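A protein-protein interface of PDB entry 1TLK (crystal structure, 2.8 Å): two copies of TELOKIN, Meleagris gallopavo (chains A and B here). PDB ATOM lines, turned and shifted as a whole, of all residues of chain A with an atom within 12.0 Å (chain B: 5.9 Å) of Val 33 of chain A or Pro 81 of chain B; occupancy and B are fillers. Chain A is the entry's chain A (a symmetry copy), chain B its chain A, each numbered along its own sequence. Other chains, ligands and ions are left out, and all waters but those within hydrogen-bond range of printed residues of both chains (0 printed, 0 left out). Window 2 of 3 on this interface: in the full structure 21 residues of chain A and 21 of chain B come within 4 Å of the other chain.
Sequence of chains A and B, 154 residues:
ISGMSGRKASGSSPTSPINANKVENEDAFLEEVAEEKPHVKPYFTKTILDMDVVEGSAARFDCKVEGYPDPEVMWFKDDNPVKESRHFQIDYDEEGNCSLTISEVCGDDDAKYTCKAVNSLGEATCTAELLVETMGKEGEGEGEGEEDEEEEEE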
ATOM      1  N   VAL A  33     -22.221 -11.271 -15.112  1.00  0.00           N
ATOM      2  CA  VAL A  33     -22.169 -10.946 -13.695  1.00  0.00           C
ATOM      3  C   VAL A  33     -22.414 -12.249 -12.903  1.00  0.00           C
ATOM      4  O   VAL A  33     -23.541 -12.735 -12.944  1.00  0.00           O
ATOM      5  CB  VAL A  33     -23.229  -9.871 -13.498  1.00  0.00           C
ATOM      6  CG1 VAL A  33     -23.773  -9.892 -12.081  1.00  0.00           C
ATOM      7  CG2 VAL A  33     -22.649  -8.495 -13.803  1.00  0.00           C
ATOM      8  N   ALA A  34     -21.400 -12.881 -12.240  1.00  0.00           N
ATOM      9  CA  ALA A  34     -21.666 -14.170 -11.567  1.00  0.00           C
ATOM     10  C   ALA A  34     -20.972 -14.622 -10.286  1.00  0.00           C
ATOM     11  O   ALA A  34     -19.757 -14.779 -10.201  1.00  0.00           O
ATOM     12  CB  ALA A  34     -21.736 -15.306 -12.575  1.00  0.00           C
ATOM     13  N   GLU A  35     -21.814 -14.885  -9.300  1.00  0.00           N
ATOM     14  CA  GLU A  35     -21.321 -15.320  -8.023  1.00  0.00           C
ATOM     15  C   GLU A  35     -21.200 -16.834  -7.850  1.00  0.00           C
ATOM     16  O   GLU A  35     -22.094 -17.590  -8.240  1.00  0.00           O
ATOM     17  CB  GLU A  35     -21.961 -14.535  -6.844  1.00  0.00           C
ATOM     18  CG  GLU A  35     -20.861 -13.865  -5.975  1.00  0.00           C
ATOM     19  CD  GLU A  35     -21.216 -13.199  -4.654  1.00  0.00           C
ATOM     20  OE1 GLU A  35     -21.926 -12.209  -4.557  1.00  0.00           O
ATOM     21  OE2 GLU A  35     -20.607 -13.747  -3.626  1.00  0.00           O
ATOM     22  N   GLU A  36     -20.048 -17.233  -7.268  1.00  0.00           N
ATOM     23  CA  GLU A  36     -19.637 -18.609  -6.951  1.00  0.00           C
ATOM     24  C   GLU A  36     -19.579 -18.807  -5.431  1.00  0.00           C
ATOM     25  O   GLU A  36     -19.219 -17.888  -4.696  1.00  0.00           O
ATOM     26  CB  GLU A  36     -18.348 -19.136  -7.713  1.00  0.00           C
ATOM     27  CG  GLU A  36     -17.119 -19.610  -6.844  1.00  0.00           C
ATOM     28  CD  GLU A  36     -16.067 -20.651  -7.313  1.00  0.00           C
ATOM     29  OE1 GLU A  36     -16.541 -21.667  -7.996  1.00  0.00           O
ATOM     30  OE2 GLU A  36     -14.884 -20.577  -6.988  1.00  0.00           O
ATOM     31  N   LYS A  37     -19.930 -19.999  -4.946  1.00  0.00           N
ATOM     32  CA  LYS A  37     -19.886 -20.264  -3.516  1.00  0.00           C
ATOM     33  C   LYS A  37     -18.520 -19.952  -2.936  1.00  0.00           C
ATOM     34  O   LYS A  37     -17.520 -19.919  -3.641  1.00  0.00           O
ATOM     35  CB  LYS A  37     -20.241 -21.694  -3.188  1.00  0.00           C
ATOM     36  CG  LYS A  37     -21.723 -21.878  -2.950  1.00  0.00           C
ATOM     37  CD  LYS A  37     -22.210 -23.272  -3.325  1.00  0.00           C
ATOM     38  CE  LYS A  37     -22.976 -23.880  -2.162  1.00  0.00           C
ATOM     39  NZ  LYS A  37     -23.961 -24.957  -2.586  1.00  0.00           N
ATOM     40  N   VAL B  73     -24.855 -17.937  -9.450  1.00  0.00           N
ATOM     41  CA  VAL B  73     -25.907 -17.040  -9.208  1.00  0.00           C
ATOM     42  C   VAL B  73     -25.660 -15.625  -9.590  1.00  0.00           C
ATOM     43  O   VAL B  73     -24.633 -15.030  -9.260  1.00  0.00           O
ATOM     44  CB  VAL B  73     -26.187 -17.066  -7.725  1.00  0.00           C
ATOM     45  CG1 VAL B  73     -27.555 -16.456  -7.460  1.00  0.00           C
ATOM     46  CG2 VAL B  73     -26.146 -18.503  -7.224  1.00  0.00           C
ATOM     47  N   MET B  74     -26.707 -15.137 -10.255  1.00  0.00           N
ATOM     48  CA  MET B  74     -26.851 -13.794 -10.757  1.00  0.00           C
ATOM     49  C   MET B  74     -28.220 -13.203 -10.430  1.00  0.00           C
ATOM     50  O   MET B  74     -29.261 -13.865 -10.468  1.00  0.00           O
ATOM     51  CB  MET B  74     -26.593 -13.708 -12.263  1.00  0.00           C
ATOM     52  CG  MET B  74     -26.784 -15.105 -12.799  1.00  0.00           C
ATOM     53  SD  MET B  74     -26.183 -15.409 -14.466  1.00  0.00           S
ATOM     54  CE  MET B  74     -26.774 -17.119 -14.625  1.00  0.00           C
ATOM     55  N   TRP B  75     -28.153 -11.910 -10.122  1.00  0.00           N
ATOM     56  CA  TRP B  75     -29.271 -11.054  -9.804  1.00  0.00           C
ATOM     57  C   TRP B  75     -29.455 -10.035 -10.924  1.00  0.00           C
ATOM     58  O   TRP B  75     -28.518  -9.586 -11.594  1.00  0.00           O
ATOM     59  CB  TRP B  75     -29.111 -10.354  -8.443  1.00  0.00           C
ATOM     60  CG  TRP B  75     -29.150 -11.281  -7.270  1.00  0.00           C
ATOM     61  CD1 TRP B  75     -28.137 -12.041  -6.785  1.00  0.00           C
ATOM     62  CD2 TRP B  75     -30.275 -11.515  -6.435  1.00  0.00           C
ATOM     63  NE1 TRP B  75     -28.569 -12.759  -5.703  1.00  0.00           N
ATOM     64  CE2 TRP B  75     -29.878 -12.448  -5.461  1.00  0.00           C
ATOM     65  CE3 TRP B  75     -31.571 -11.022  -6.429  1.00  0.00           C
ATOM     66  CZ2 TRP B  75     -30.746 -12.888  -4.471  1.00  0.00           C
ATOM     67  CZ3 TRP B  75     -32.429 -11.456  -5.451  1.00  0.00           C
ATOM     68  CH2 TRP B  75     -32.024 -12.383  -4.488  1.00  0.00           C
ATOM     69  N   PHE B  76     -30.714  -9.698 -11.094  1.00  0.00           N
ATOM     70  CA  PHE B  76     -31.149  -8.770 -12.091  1.00  0.00           C
ATOM     71  C   PHE B  76     -32.200  -7.864 -11.506  1.00  0.00           C
ATOM     72  O   PHE B  76     -32.982  -8.245 -10.637  1.00  0.00           O
ATOM     73  CB  PHE B  76     -31.825  -9.541 -13.247  1.00  0.00           C
ATOM     74  CG  PHE B  76     -30.920 -10.528 -13.951  1.00  0.00           C
ATOM     75  CD1 PHE B  76     -30.659 -11.803 -13.446  1.00  0.00           C
ATOM     76  CD2 PHE B  76     -30.261 -10.169 -15.124  1.00  0.00           C
ATOM     77  CE1 PHE B  76     -29.813 -12.697 -14.105  1.00  0.00           C
ATOM     78  CE2 PHE B  76     -29.395 -11.037 -15.793  1.00  0.00           C
ATOM     79  CZ  PHE B  76     -29.181 -12.322 -15.290  1.00  0.00           C
ATOM     80  N   LYS B  77     -32.208  -6.664 -12.056  1.00  0.00           N
ATOM     81  CA  LYS B  77     -33.137  -5.619 -11.728  1.00  0.00           C
ATOM     82  C   LYS B  77     -33.787  -5.199 -13.014  1.00  0.00           C
ATOM     83  O   LYS B  77     -33.219  -4.429 -13.794  1.00  0.00           O
ATOM     84  CB  LYS B  77     -32.494  -4.393 -11.110  1.00  0.00           C
ATOM     85  CG  LYS B  77     -33.478  -3.420 -10.484  1.00  0.00           C
ATOM     86  CD  LYS B  77     -32.733  -2.238  -9.900  1.00  0.00           C
ATOM     87  CE  LYS B  77     -32.721  -1.053 -10.840  1.00  0.00           C
ATOM     88  NZ  LYS B  77     -32.789   0.215 -10.110  1.00  0.00           N
ATOM     89  N   ASP B  79     -34.619  -6.951 -15.943  1.00  0.00           N
ATOM     90  CA  ASP B  79     -33.946  -7.407 -17.136  1.00  0.00           C
ATOM     91  C   ASP B  79     -32.442  -7.063 -17.165  1.00  0.00           C
ATOM     92  O   ASP B  79     -31.715  -7.545 -18.033  1.00  0.00           O
ATOM     93  CB  ASP B  79     -34.678  -6.795 -18.371  1.00  0.00           C
ATOM     94  CG  ASP B  79     -35.834  -7.567 -18.976  1.00  0.00           C
ATOM     95  OD1 ASP B  79     -36.838  -7.893 -18.369  1.00  0.00           O
ATOM     96  OD2 ASP B  79     -35.626  -7.850 -20.238  1.00  0.00           O
ATOM     97  N   ASN B  80     -31.982  -6.229 -16.215  1.00  0.00           N
ATOM     98  CA  ASN B  80     -30.603  -5.737 -16.082  1.00  0.00           C
ATOM     99  C   ASN B  80     -29.762  -6.409 -14.997  1.00  0.00           C
ATOM    100  O   ASN B  80     -30.224  -6.612 -13.878  1.00  0.00           O
ATOM    101  CB  ASN B  80     -30.700  -4.250 -15.686  1.00  0.00           C
ATOM    102  CG  ASN B  80     -29.934  -3.278 -16.556  1.00  0.00           C
ATOM    103  OD1 ASN B  80     -29.733  -2.117 -16.171  1.00  0.00           O
ATOM    104  ND2 ASN B  80     -29.517  -3.738 -17.730  1.00  0.00           N
ATOM    105  N   PRO B  81     -28.510  -6.713 -15.304  1.00  0.00           N
ATOM    106  CA  PRO B  81     -27.624  -7.336 -14.341  1.00  0.00           C
ATOM    107  C   PRO B  81     -27.341  -6.449 -13.148  1.00  0.00           C
ATOM    108  O   PRO B  81     -27.307  -5.224 -13.228  1.00  0.00           O
ATOM    109  CB  PRO B  81     -26.327  -7.647 -15.081  1.00  0.00           C
ATOM    110  CG  PRO B  81     -26.560  -7.309 -16.548  1.00  0.00           C
ATOM    111  CD  PRO B  81     -27.891  -6.585 -16.644  1.00  0.00           C
ATOM    112  N   VAL B  82     -27.164  -7.094 -12.021  1.00  0.00           N
ATOM    113  CA  VAL B  82     -26.894  -6.328 -10.845  1.00  0.00           C
ATOM    114  C   VAL B  82     -25.453  -6.527 -10.439  1.00  0.00           C
ATOM    115  O   VAL B  82     -25.050  -7.638 -10.101  1.00  0.00           O
ATOM    116  CB  VAL B  82     -27.768  -6.757  -9.680  1.00  0.00           C
ATOM    117  CG1 VAL B  82     -27.092  -6.310  -8.401  1.00  0.00           C
ATOM    118  CG2 VAL B  82     -29.120  -6.061  -9.726  1.00  0.00           C
ATOM    119  N   LYS B  83     -24.683  -5.443 -10.470  1.00  0.00           N
ATOM    120  CA  LYS B  83     -23.284  -5.464 -10.083  1.00  0.00           C
ATOM    121  C   LYS B  83     -23.231  -4.995  -8.647  1.00  0.00           C
ATOM    122  O   LYS B  83     -23.801  -3.973  -8.259  1.00  0.00           O
ATOM    123  CB  LYS B  83     -22.398  -4.554 -10.962  1.00  0.00           C
ATOM    124  CG  LYS B  83     -21.000  -5.045 -11.408  1.00  0.00           C
ATOM    125  CD  LYS B  83     -20.038  -3.973 -12.001  1.00  0.00           C
ATOM    126  CE  LYS B  83     -19.619  -4.039 -13.492  1.00  0.00           C
ATOM    127  NZ  LYS B  83     -19.074  -2.756 -13.994  1.00  0.00           N
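Among the printed residues, pairs that only touch across the chains: Val 33 of chain A with Met 74 of chain B, Val 33 of chain A with Pro 81 of chain B, Val 33 of chain A with Val 82 of chain B and Ala 34 of chain A with Val 73 of chain B.
No position is printed for both chains.
N of Glu 35 of chain A is in hydrogen-bond range of O of Val 73 of chain B (2.8 Å).
Of the printed residues of chain B, Val 33 of chain A touches Met 74 (3.3 Å), Pro 81 (3.98 Å) and Val 82 (3.3 Å).
Printed residues of chain B within 4 Å of Ala 34 of chain A: Val 73 (3.8 Å).
Printed residues of chain B within 4 Å of Glu 35 of chain A: Val 73.
Of the printed residues of chain A, Val 73 of chain B touches Ala 34 (3.8 Å) and Glu 35 (2.8 Å).
Met 74 of chain B touches just one residue of chain A: Val 33.
No residue of chain A comes within 4 Å of Asn 80 of chain B.
Printed residues of chain A within 4 Å of Pro 81 of chain B: Val 33 (3.98 Å).
Of chain A, only Val 33 (3.3 Å) comes within 4 Å of Val 82 of chain B.
No residue of chain A comes within 4 Å of Lys 83 of chain B.
Of the 5 printed residues of chain A, 3 touch a printed residue of chain B.
Printed residues of chain A that touch a printed residue of chain B: Val 33, Ala 34 and Glu 35.
Hydrophobic or aromatic side chains of chain A that line the printed part of chain B: Val 33.
Hydrophobic or aromatic side chains of chain B within 4 Å of the printed part of chain A: Met 74 and Pro 81.
Among the printed residues, no Asp or Glu carboxylate lies within 4 Å of a Lys or Arg side-chain nitrogen of the other chain.
O of Trp 75 of chain B lies within hydrogen-bond range of N of Val 82 of chain B (2.9 Å).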
